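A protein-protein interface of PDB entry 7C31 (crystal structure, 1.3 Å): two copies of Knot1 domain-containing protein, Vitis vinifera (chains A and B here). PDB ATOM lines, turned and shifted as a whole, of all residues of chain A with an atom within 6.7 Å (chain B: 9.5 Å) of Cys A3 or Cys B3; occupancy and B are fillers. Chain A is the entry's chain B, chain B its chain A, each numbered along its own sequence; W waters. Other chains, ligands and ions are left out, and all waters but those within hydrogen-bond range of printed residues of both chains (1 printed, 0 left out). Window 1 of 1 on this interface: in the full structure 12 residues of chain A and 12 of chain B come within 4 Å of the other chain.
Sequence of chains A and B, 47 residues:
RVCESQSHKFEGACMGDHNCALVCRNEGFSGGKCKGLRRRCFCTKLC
Hydrophobic or aromatic side chains of chain A that line the printed part of chain B: Phe A29.
Along chain A the printed residues that touch a printed residue of chain B span positions 1 to 47.
Among the printed residues, 20 pairs touch across the chains.
Among the printed residues, Asp or Glu carboxylates within 4 Å of a Lys or Arg side-chain nitrogen of the other chain: Arg A1 with Glu B27.
Val A2 touches Ser B5, and with the chains exchanged Ser A5 touches Val B2.
Cys A3 touches Phe B29, and with the chains exchanged Phe A29 touches Cys B3.
Glu A4 touches its own counterpart, Glu B4.
Cys A47 touches Cys B3, but with the chains exchanged Cys A3 does not touch Cys B47 (6.2 Å).
Positions printed for both chains: 1, 2, 3, 4, 5, 29, 43, 44, 45, 46 and 47.
Phe B29 touches Arg A1 (CE1 to CZ, 3.4 Å).
Cys A3 touches Cys B3.
CA of Cys A3 touches O of Glu B4 (3.3 Å).
Cys A3 touches Ser B5 (SG to CB, 3.9 Å).
Phe B29 touches Cys A3 (CE2 to SG, 3.8 Å).
Cys B3 touches Glu A4 (CA to O, 3.3 Å).
Phe A29 touches Arg B1 (CE1 to CZ, 3.6 Å).
Phe A29 touches Cys B3 (CE2 to SG, 3.9 Å).
Phe A29 touches Cys B47 (CZ to SG, 3.97 Å).
Cys A47 touches Cys B3 (SG to CB, 3.995 Å).
Printed residues of chain A within 4 Å of Cys B3: Cys A3, Glu A4, Phe A29 and Cys A47.
No residue of chain B comes within 4 Å of Thr A44.
Of the printed residues of chain A, Arg B1 touches Ser A5 and Phe A29.
Of the printed residues of chain A, Val B2 touches Ser A5 (2.8 Å).
Of the printed residues of chain B, Cys A47 touches Cys B3 and Lys B45.
The nearest printed residue of chain A that does not touch Cys B3 is Ser A5 (4.02 Å).
Water W1 bridges the backbone carbonyl oxygen (O) of Glu B27 (3.0 Å) and the guanidinium group (NH1) of Arg A1 (3.3 Å).
The backbone carbonyl oxygen (O) of Arg B1 sits at hydrogen-bond distance from the backbone NH (N) of Cys B47 (2.7 Å).
N of Cys B3 sits at hydrogen-bond distance from O of Lys B45.
O of Cys B24 is in hydrogen-bond range of N of Phe B29 (3.0 Å).
O of Arg A1 is in hydrogen-bond range of N of Cys A47, at 3.0 Å.
O of Lys A45 is in hydrogen-bond range of N of Cys A3, at 2.9 Å.
SG of Cys A47 is disulfide-bonded to SG of Cys A3 (2.0 Å).
NE of Arg B1 lies within hydrogen-bond range of OG of Ser A5 (3.0 Å).
O of Val B2 lies within hydrogen-bond range of OG of Ser A5, at 2.8 Å.
N of Glu A4 lies within hydrogen-bond range of O of Glu B4 (2.9 Å).
NE of Arg A1 is in hydrogen-bond range of OG of Ser B5, at 2.8 Å.
The side-chain hydroxyl of Ser B5 is in hydrogen-bond range of the backbone carbonyl oxygen of Val A2, 3.0 Å away.
The backbone carbonyl oxygen (O) of Gln B6 lies within hydrogen-bond range of the guanidinium group (NH2) of Arg A1 (2.8 Å).
NE2 of His B8 sits at hydrogen-bond distance from NE of Arg A1, 3.5 Å away.
The side-chain carboxylate (OE1) of Glu B27 is in salt-bridge range of the guanidinium group (NH2) of Arg A1, 3.0 Å away.
The side-chain amino group (NZ) of Lys B45 lies within salt-bridge range of the chain-end carboxylate (O) of Cys A47, at 3.5 Å.
The side-chain amino group of Lys A45 is in salt-bridge range of the chain-end carboxylate of Cys B47 (3.2 Å).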
ATOM      1  N   ARG A   1     -12.201  20.548  20.856  1.00  0.00           N
ATOM      2  CA  ARG A   1     -13.197  21.637  21.083  1.00  0.00           C
ATOM      3  C   ARG A   1     -12.536  22.994  20.858  1.00  0.00           C
ATOM      4  O   ARG A   1     -11.601  23.351  21.582  1.00  0.00           O
ATOM      5  CB  ARG A   1     -13.755  21.537  22.502  1.00  0.00           C
ATOM      6  CG  ARG A   1     -14.783  22.597  22.869  1.00  0.00           C
ATOM      7  CD  ARG A   1     -16.141  22.226  22.353  1.00  0.00           C
ATOM      8  NE  ARG A   1     -17.198  23.137  22.780  1.00  0.00           N
ATOM      9  CZ  ARG A   1     -18.078  22.868  23.741  1.00  0.00           C
ATOM     10  NH1 ARG A   1     -18.019  21.730  24.421  1.00  0.00           N
ATOM     11  NH2 ARG A   1     -19.017  23.760  24.026  1.00  0.00           N
ATOM     12  N   VAL A   2     -13.038  23.757  19.837  1.00  0.00           N
ATOM     13  CA  VAL A   2     -12.493  25.061  19.484  1.00  0.00           C
ATOM     14  C   VAL A   2     -13.232  26.149  20.245  1.00  0.00           C
ATOM     15  O   VAL A   2     -14.435  26.042  20.524  1.00  0.00           O
ATOM     16  CB  VAL A   2     -12.590  25.288  17.959  1.00  0.00           C
ATOM     17  CG1 VAL A   2     -14.046  25.398  17.519  1.00  0.00           C
ATOM     18  CG2 VAL A   2     -11.828  26.548  17.530  1.00  0.00           C
ATOM     19  N   CYS A   3     -12.508  27.213  20.557  1.00  0.00           N
ATOM     20  CA  CYS A   3     -13.063  28.418  21.139  1.00  0.00           C
ATOM     21  C   CYS A   3     -12.627  29.628  20.339  1.00  0.00           C
ATOM     22  O   CYS A   3     -11.604  29.609  19.641  1.00  0.00           O
ATOM     23  CB  CYS A   3     -12.560  28.664  22.554  1.00  0.00           C
ATOM     24  SG  CYS A   3     -13.028  27.465  23.727  1.00  0.00           S
ATOM     25  N   GLU A   4     -13.360  30.715  20.529  1.00  0.00           N
ATOM     26  CA  GLU A   4     -13.184  31.947  19.779  1.00  0.00           C
ATOM     27  C   GLU A   4     -13.098  33.147  20.699  1.00  0.00           C
ATOM     28  O   GLU A   4     -13.736  33.185  21.746  1.00  0.00           O
ATOM     29  CB  GLU A   4     -14.380  32.107  18.876  1.00  0.00           C
ATOM     30  CG  GLU A   4     -14.249  33.083  17.798  1.00  0.00           C
ATOM     31  CD  GLU A   4     -15.406  32.931  16.876  1.00  0.00           C
ATOM     32  OE1 GLU A   4     -16.537  33.220  17.323  1.00  0.00           O
ATOM     33  OE2 GLU A   4     -15.187  32.464  15.741  1.00  0.00           O
ATOM     34  N   SER A   5     -12.323  34.141  20.266  1.00  0.00           N
ATOM     35  CA  SER A   5     -12.196  35.395  21.006  1.00  0.00           C
ATOM     36  C   SER A   5     -11.919  36.514  20.018  1.00  0.00           C
ATOM     37  O   SER A   5     -10.990  36.395  19.217  1.00  0.00           O
ATOM     38  CB  SER A   5     -11.028  35.313  21.986  1.00  0.00           C
ATOM     39  OG  SER A   5     -10.976  36.461  22.807  1.00  0.00           O
ATOM     40  N   PHE A  29      -3.146  32.645  19.470  1.00  0.00           N
ATOM     41  CA  PHE A  29      -4.181  31.760  18.961  1.00  0.00           C
ATOM     42  C   PHE A  29      -3.641  30.981  17.770  1.00  0.00           C
ATOM     43  O   PHE A  29      -2.564  31.274  17.255  1.00  0.00           O
ATOM     44  CB  PHE A  29      -5.366  32.623  18.591  1.00  0.00           C
ATOM     45  CG  PHE A  29      -6.102  33.128  19.766  1.00  0.00           C
ATOM     46  CD1 PHE A  29      -5.651  34.241  20.477  1.00  0.00           C
ATOM     47  CD2 PHE A  29      -7.212  32.482  20.189  1.00  0.00           C
ATOM     48  CE1 PHE A  29      -6.344  34.658  21.594  1.00  0.00           C
ATOM     49  CE2 PHE A  29      -7.904  32.893  21.309  1.00  0.00           C
ATOM     50  CZ  PHE A  29      -7.471  33.990  21.998  1.00  0.00           C
ATOM     51  N   CYS A  43     -10.327  35.385  16.651  1.00  0.00           N
ATOM     52  CA  CYS A  43      -9.231  34.431  16.801  1.00  0.00           C
ATOM     53  C   CYS A  43      -9.808  33.127  17.336  1.00  0.00           C
ATOM     54  O   CYS A  43     -10.808  33.115  18.067  1.00  0.00           O
ATOM     55  CB  CYS A  43      -8.226  34.979  17.784  1.00  0.00           C
ATOM     56  SG  CYS A  43      -7.536  36.600  17.272  1.00  0.00           S
ATOM     57  N   THR A  44      -9.178  32.014  16.965  1.00  0.00           N
ATOM     58  CA  THR A  44      -9.609  30.691  17.421  1.00  0.00           C
ATOM     59  C   THR A  44      -8.429  29.892  17.960  1.00  0.00           C
ATOM     60  O   THR A  44      -7.291  30.056  17.500  1.00  0.00           O
ATOM     61  CB  THR A  44     -10.300  29.893  16.298  1.00  0.00           C
ATOM     62  OG1 THR A  44      -9.483  29.886  15.123  1.00  0.00           O
ATOM     63  CG2 THR A  44     -11.659  30.492  15.974  1.00  0.00           C
ATOM     64  N   LYS A  45      -8.711  29.009  18.905  1.00  0.00           N
ATOM     65  CA  LYS A  45      -7.721  28.075  19.430  1.00  0.00           C
ATOM     66  C   LYS A  45      -8.470  26.928  20.084  1.00  0.00           C
ATOM     67  O   LYS A  45      -9.681  26.989  20.266  1.00  0.00           O
ATOM     68  CB  LYS A  45      -6.792  28.737  20.460  1.00  0.00           C
ATOM     69  CG  LYS A  45      -7.491  29.126  21.768  1.00  0.00           C
ATOM     70  CD  LYS A  45      -6.577  29.825  22.788  1.00  0.00           C
ATOM     71  CE  LYS A  45      -5.696  28.864  23.582  1.00  0.00           C
ATOM     72  NZ  LYS A  45      -4.875  29.577  24.621  1.00  0.00           N
ATOM     73  N   LEU A  46      -7.748  25.881  20.473  1.00  0.00           N
ATOM     74  CA  LEU A  46      -8.387  24.834  21.240  1.00  0.00           C
ATOM     75  C   LEU A  46      -8.566  25.310  22.670  1.00  0.00           C
ATOM     76  O   LEU A  46      -7.643  25.877  23.266  1.00  0.00           O
ATOM     77  CB  LEU A  46      -7.521  23.570  21.317  1.00  0.00           C
ATOM     78  CG  LEU A  46      -7.366  22.566  20.154  1.00  0.00           C
ATOM     79  CD1 LEU A  46      -8.661  21.781  19.959  1.00  0.00           C
ATOM     80  CD2 LEU A  46      -6.865  23.347  18.837  1.00  0.00           C
ATOM     81  N   CYS A  47      -9.737  25.087  23.241  1.00  0.00           N
ATOM     82  CA  CYS A  47      -9.821  25.516  24.626  1.00  0.00           C
ATOM     83  C   CYS A  47      -9.237  24.507  25.581  1.00  0.00           C
ATOM     84  O   CYS A  47      -9.139  24.783  26.781  1.00  0.00           O
ATOM     85  CB  CYS A  47     -11.226  25.839  25.071  1.00  0.00           C
ATOM     86  SG  CYS A  47     -11.486  27.547  25.001  1.00  0.00           S
ATOM     87  OXT CYS A  47      -8.893  23.417  25.146  1.00  0.00           O
ATOM     88  N   ARG B   1      -8.413  37.253  29.430  1.00  0.00           N
ATOM     89  CA  ARG B   1      -9.015  37.169  28.068  1.00  0.00           C
ATOM     90  C   ARG B   1     -10.020  36.035  27.979  1.00  0.00           C
ATOM     91  O   ARG B   1      -9.715  34.896  28.342  1.00  0.00           O
ATOM     92  CB  ARG B   1      -7.940  36.971  27.023  1.00  0.00           C
ATOM     93  CG  ARG B   1      -8.542  36.909  25.671  1.00  0.00           C
ATOM     94  CD  ARG B   1      -7.565  37.347  24.674  1.00  0.00           C
ATOM     95  NE  ARG B   1      -8.200  37.427  23.377  1.00  0.00           N
ATOM     96  CZ  ARG B   1      -7.593  37.905  22.305  1.00  0.00           C
ATOM     97  NH1 ARG B   1      -6.345  38.338  22.413  1.00  0.00           N
ATOM     98  NH2 ARG B   1      -8.231  37.948  21.147  1.00  0.00           N
ATOM     99  N   VAL B   2     -11.217  36.358  27.470  1.00  0.00           N
ATOM    100  CA  VAL B   2     -12.356  35.444  27.452  1.00  0.00           C
ATOM    101  C   VAL B   2     -12.477  34.790  26.087  1.00  0.00           C
ATOM    102  O   VAL B   2     -12.389  35.462  25.047  1.00  0.00           O
ATOM    103  CB  VAL B   2     -13.666  36.166  27.817  1.00  0.00           C
ATOM    104  CG1 VAL B   2     -14.867  35.194  27.770  1.00  0.00           C
ATOM    105  CG2 VAL B   2     -13.514  36.842  29.174  1.00  0.00           C
ATOM    106  N   CYS B   3     -12.692  33.483  26.112  1.00  0.00           N
ATOM    107  CA  CYS B   3     -13.001  32.663  24.954  1.00  0.00           C
ATOM    108  C   CYS B   3     -14.406  32.096  25.101  1.00  0.00           C
ATOM    109  O   CYS B   3     -14.895  31.875  26.206  1.00  0.00           O
ATOM    110  CB  CYS B   3     -12.006  31.506  24.866  1.00  0.00           C
ATOM    111  SG  CYS B   3     -10.426  31.932  24.082  1.00  0.00           S
ATOM    112  N   GLU B   4     -15.042  31.866  23.956  1.00  0.00           N
ATOM    113  CA  GLU B   4     -16.396  31.363  23.875  1.00  0.00           C
ATOM    114  C   GLU B   4     -16.491  30.180  22.927  1.00  0.00           C
ATOM    115  O   GLU B   4     -15.789  30.105  21.909  1.00  0.00           O
ATOM    116  CB  GLU B   4     -17.389  32.396  23.338  1.00  0.00           C
ATOM    117  CG  GLU B   4     -17.875  33.442  24.314  1.00  0.00           C
ATOM    118  CD  GLU B   4     -18.996  34.266  23.703  1.00  0.00           C
ATOM    119  OE1 GLU B   4     -19.213  34.147  22.475  1.00  0.00           O
ATOM    120  OE2 GLU B   4     -19.660  35.019  24.445  1.00  0.00           O
ATOM    121  N   SER B   5     -17.426  29.282  23.242  1.00  0.00           N
ATOM    122  CA  SER B   5     -17.703  28.117  22.404  1.00  0.00           C
ATOM    123  C   SER B   5     -19.174  27.777  22.590  1.00  0.00           C
ATOM    124  O   SER B   5     -19.636  27.660  23.723  1.00  0.00           O
ATOM    125  CB  SER B   5     -16.844  26.946  22.885  1.00  0.00           C
ATOM    126  OG  SER B   5     -17.002  25.826  22.034  1.00  0.00           O
ATOM    127  N   GLN B   6     -19.904  27.598  21.508  1.00  0.00           N
ATOM    128  CA  GLN B   6     -21.298  27.200  21.645  1.00  0.00           C
ATOM    129  C   GLN B   6     -21.400  25.863  22.375  1.00  0.00           C
ATOM    130  O   GLN B   6     -20.639  24.922  22.119  1.00  0.00           O
ATOM    131  CB  GLN B   6     -21.955  27.077  20.279  1.00  0.00           C
ATOM    132  CG  GLN B   6     -23.468  26.957  20.355  1.00  0.00           C
ATOM    133  CD  GLN B   6     -24.128  26.788  19.004  1.00  0.00           C
ATOM    134  OE1 GLN B   6     -23.553  27.122  17.969  1.00  0.00           O
ATOM    135  NE2 GLN B   6     -25.352  26.284  19.023  1.00  0.00           N
ATOM    136  N   HIS B   8     -22.475  22.207  23.405  1.00  0.00           N
ATOM    137  CA  HIS B   8     -22.883  21.002  22.683  1.00  0.00           C
ATOM    138  C   HIS B   8     -24.115  20.351  23.306  1.00  0.00           C
ATOM    139  O   HIS B   8     -24.879  19.688  22.598  1.00  0.00           O
ATOM    140  CB  HIS B   8     -21.753  19.962  22.615  1.00  0.00           C
ATOM    141  CG  HIS B   8     -20.628  20.352  21.712  1.00  0.00           C
ATOM    142  ND1 HIS B   8     -19.795  19.440  21.107  1.00  0.00           N
ATOM    143  CD2 HIS B   8     -20.199  21.569  21.305  1.00  0.00           C
ATOM    144  CE1 HIS B   8     -18.905  20.079  20.367  1.00  0.00           C
ATOM    145  NE2 HIS B   8     -19.127  21.370  20.473  1.00  0.00           N
ATOM    146  N   CYS B  24     -22.948  24.587  30.719  1.00  0.00           N
ATOM    147  CA  CYS B  24     -21.582  24.829  30.261  1.00  0.00           C
ATOM    148  C   CYS B  24     -20.551  24.358  31.286  1.00  0.00           C
ATOM    149  O   CYS B  24     -19.493  23.835  30.919  1.00  0.00           O
ATOM    150  CB  CYS B  24     -21.431  26.326  29.991  1.00  0.00           C
ATOM    151  SG  CYS B  24     -22.214  26.841  28.474  1.00  0.00           S
ATOM    152  N   GLU B  27     -19.993  20.828  30.849  1.00  0.00           N
ATOM    153  CA  GLU B  27     -19.146  20.598  29.684  1.00  0.00           C
ATOM    154  C   GLU B  27     -17.694  21.007  29.897  1.00  0.00           C
ATOM    155  O   GLU B  27     -16.899  20.897  28.952  1.00  0.00           O
ATOM    156  CB  GLU B  27     -19.652  21.411  28.485  1.00  0.00           C
ATOM    157  CG  GLU B  27     -20.994  20.970  27.968  1.00  0.00           C
ATOM    158  CD  GLU B  27     -21.504  21.747  26.761  1.00  0.00           C
ATOM    159  OE1 GLU B  27     -20.734  22.076  25.824  1.00  0.00           O
ATOM    160  OE2 GLU B  27     -22.724  21.991  26.739  1.00  0.00           O
ATOM    161  N   GLY B  28     -17.339  21.534  31.063  1.00  0.00           N
ATOM    162  CA  GLY B  28     -15.955  21.854  31.353  1.00  0.00           C
ATOM    163  C   GLY B  28     -15.580  23.314  31.257  1.00  0.00           C
ATOM    164  O   GLY B  28     -14.403  23.648  31.431  1.00  0.00           O
ATOM    165  N   PHE B  29     -16.531  24.192  30.994  1.00  0.00           N
ATOM    166  CA  PHE B  29     -16.305  25.626  30.952  1.00  0.00           C
ATOM    167  C   PHE B  29     -16.563  26.247  32.315  1.00  0.00           C
ATOM    168  O   PHE B  29     -16.974  25.574  33.261  1.00  0.00           O
ATOM    169  CB  PHE B  29     -17.178  26.227  29.851  1.00  0.00           C
ATOM    170  CG  PHE B  29     -16.744  25.852  28.438  1.00  0.00           C
ATOM    171  CD1 PHE B  29     -17.146  24.636  27.868  1.00  0.00           C
ATOM    172  CD2 PHE B  29     -15.913  26.684  27.698  1.00  0.00           C
ATOM    173  CE1 PHE B  29     -16.728  24.282  26.568  1.00  0.00           C
ATOM    174  CE2 PHE B  29     -15.473  26.331  26.427  1.00  0.00           C
ATOM    175  CZ  PHE B  29     -15.894  25.131  25.854  1.00  0.00           C
ATOM    176  N   SER B  30     -16.287  27.543  32.435  1.00  0.00           N
ATOM    177  CA  SER B  30     -16.518  28.249  33.688  1.00  0.00           C
ATOM    178  C   SER B  30     -17.910  28.854  33.800  1.00  0.00           C
ATOM    179  O   SER B  30     -18.352  29.169  34.911  1.00  0.00           O
ATOM    180  CB  SER B  30     -15.487  29.371  33.863  1.00  0.00           C
ATOM    181  OG  SER B  30     -15.712  30.413  32.928  1.00  0.00           O
ATOM    182  N   GLY B  31     -18.604  29.025  32.688  1.00  0.00           N
ATOM    183  CA  GLY B  31     -19.921  29.612  32.730  1.00  0.00           C
ATOM    184  C   GLY B  31     -20.400  29.761  31.305  1.00  0.00           C
ATOM    185  O   GLY B  31     -19.887  29.099  30.399  1.00  0.00           O
ATOM    186  N   GLY B  32     -21.375  30.634  31.119  1.00  0.00           N
ATOM    187  CA  GLY B  32     -21.962  30.804  29.804  1.00  0.00           C
ATOM    188  C   GLY B  32     -23.148  31.711  29.880  1.00  0.00           C
ATOM    189  O   GLY B  32     -23.602  32.098  30.962  1.00  0.00           O
ATOM    190  N   LYS B  33     -23.637  32.064  28.698  1.00  0.00           N
ATOM    191  CA  LYS B  33     -24.857  32.846  28.623  1.00  0.00           C
ATOM    192  C   LYS B  33     -25.522  32.665  27.271  1.00  0.00           C
ATOM    193  O   LYS B  33     -24.916  32.204  26.313  1.00  0.00           O
ATOM    194  CB  LYS B  33     -24.619  34.336  28.904  1.00  0.00           C
ATOM    195  CG  LYS B  33     -23.794  35.025  27.836  1.00  0.00           C
ATOM    196  CD  LYS B  33     -23.731  36.546  28.082  1.00  0.00           C
ATOM    197  CE  LYS B  33     -25.090  37.235  27.913  1.00  0.00           C
ATOM    198  NZ  LYS B  33     -25.374  37.809  26.557  1.00  0.00           N
ATOM    199  N   LYS B  35     -27.071  34.020  23.829  1.00  0.00           N
ATOM    200  CA  LYS B  35     -26.715  35.113  22.937  1.00  0.00           C
ATOM    201  C   LYS B  35     -27.555  35.033  21.677  1.00  0.00           C
ATOM    202  O   LYS B  35     -27.942  33.947  21.226  1.00  0.00           O
ATOM    203  CB  LYS B  35     -25.250  35.050  22.504  1.00  0.00           C
ATOM    204  CG  LYS B  35     -24.243  35.194  23.632  1.00  0.00           C
ATOM    205  CD  LYS B  35     -22.822  35.100  23.109  1.00  0.00           C
ATOM    206  CE  LYS B  35     -22.408  36.426  22.476  1.00  0.00           C
ATOM    207  NZ  LYS B  35     -21.160  36.309  21.683  1.00  0.00           N
ATOM    208  N   PHE B  42     -23.857  29.928  24.819  1.00  0.00           N
ATOM    209  CA  PHE B  42     -22.429  30.052  24.542  1.00  0.00           C
ATOM    210  C   PHE B  42     -21.657  29.949  25.845  1.00  0.00           C
ATOM    211  O   PHE B  42     -21.849  30.771  26.759  1.00  0.00           O
ATOM    212  CB  PHE B  42     -22.076  31.367  23.827  1.00  0.00           C
ATOM    213  CG  PHE B  42     -22.419  31.336  22.390  1.00  0.00           C
ATOM    214  CD1 PHE B  42     -23.683  31.653  21.945  1.00  0.00           C
ATOM    215  CD2 PHE B  42     -21.460  30.936  21.464  1.00  0.00           C
ATOM    216  CE1 PHE B  42     -24.001  31.600  20.578  1.00  0.00           C
ATOM    217  CE2 PHE B  42     -21.763  30.871  20.108  1.00  0.00           C
ATOM    218  CZ  PHE B  42     -23.033  31.195  19.673  1.00  0.00           C
ATOM    219  N   CYS B  43     -20.794  28.955  25.926  1.00  0.00           N
ATOM    220  CA  CYS B  43     -19.931  28.691  27.071  1.00  0.00           C
ATOM    221  C   CYS B  43     -18.705  29.592  27.017  1.00  0.00           C
ATOM    222  O   CYS B  43     -18.227  29.953  25.964  1.00  0.00           O
ATOM    223  CB  CYS B  43     -19.507  27.242  27.065  1.00  0.00           C
ATOM    224  SG  CYS B  43     -20.913  26.092  27.074  1.00  0.00           S
ATOM    225  N   THR B  44     -18.204  29.961  28.186  1.00  0.00           N
ATOM    226  CA  THR B  44     -17.096  30.868  28.328  1.00  0.00           C
ATOM    227  C   THR B  44     -16.048  30.339  29.287  1.00  0.00           C
ATOM    228  O   THR B  44     -16.355  29.611  30.231  1.00  0.00           O
ATOM    229  CB  THR B  44     -17.588  32.224  28.870  1.00  0.00           C
ATOM    230  OG1 THR B  44     -18.339  31.995  30.057  1.00  0.00           O
ATOM    231  CG2 THR B  44     -18.466  32.925  27.857  1.00  0.00           C
ATOM    232  N   LYS B  45     -14.801  30.724  29.045  1.00  0.00           N
ATOM    233  CA  LYS B  45     -13.715  30.462  29.977  1.00  0.00           C
ATOM    234  C   LYS B  45     -12.593  31.441  29.636  1.00  0.00           C
ATOM    235  O   LYS B  45     -12.627  32.113  28.610  1.00  0.00           O
ATOM    236  CB  LYS B  45     -13.237  29.023  29.848  1.00  0.00           C
ATOM    237  CG  LYS B  45     -12.638  28.732  28.494  1.00  0.00           C
ATOM    238  CD  LYS B  45     -12.332  27.254  28.404  1.00  0.00           C
ATOM    239  CE  LYS B  45     -11.153  26.907  29.294  1.00  0.00           C
ATOM    240  NZ  LYS B  45      -9.938  27.542  28.717  1.00  0.00           N
ATOM    241  N   LEU B  46     -11.604  31.530  30.511  1.00  0.00           N
ATOM    242  CA  LEU B  46     -10.414  32.265  30.211  1.00  0.00           C
ATOM    243  C   LEU B  46      -9.630  31.547  29.138  1.00  0.00           C
ATOM    244  O   LEU B  46      -9.545  30.326  29.150  1.00  0.00           O
ATOM    245  CB  LEU B  46      -9.550  32.288  31.424  1.00  0.00           C
ATOM    246  CG  LEU B  46      -9.771  33.538  32.207  1.00  0.00           C
ATOM    247  CD1 LEU B  46     -10.510  34.773  32.154  1.00  0.00           C
ATOM    248  CD2 LEU B  46      -9.314  33.281  33.809  1.00  0.00           C
ATOM    249  N   CYS B  47      -9.060  32.284  28.196  1.00  0.00           N
ATOM    250  CA  CYS B  47      -8.317  31.602  27.146  1.00  0.00           C
ATOM    251  C   CYS B  47      -7.058  30.996  27.751  1.00  0.00           C
ATOM    252  O   CYS B  47      -6.489  31.543  28.698  1.00  0.00           O
ATOM    253  CB  CYS B  47      -8.019  32.553  26.003  1.00  0.00           C
ATOM    254  SG  CYS B  47      -9.535  33.295  25.323  1.00  0.00           S
ATOM    255  OXT CYS B  47      -6.609  29.925  27.334  1.00  0.00           O
HETATM  256  O   HOH W   1     -16.324  19.617  26.245  1.00  0.00           O
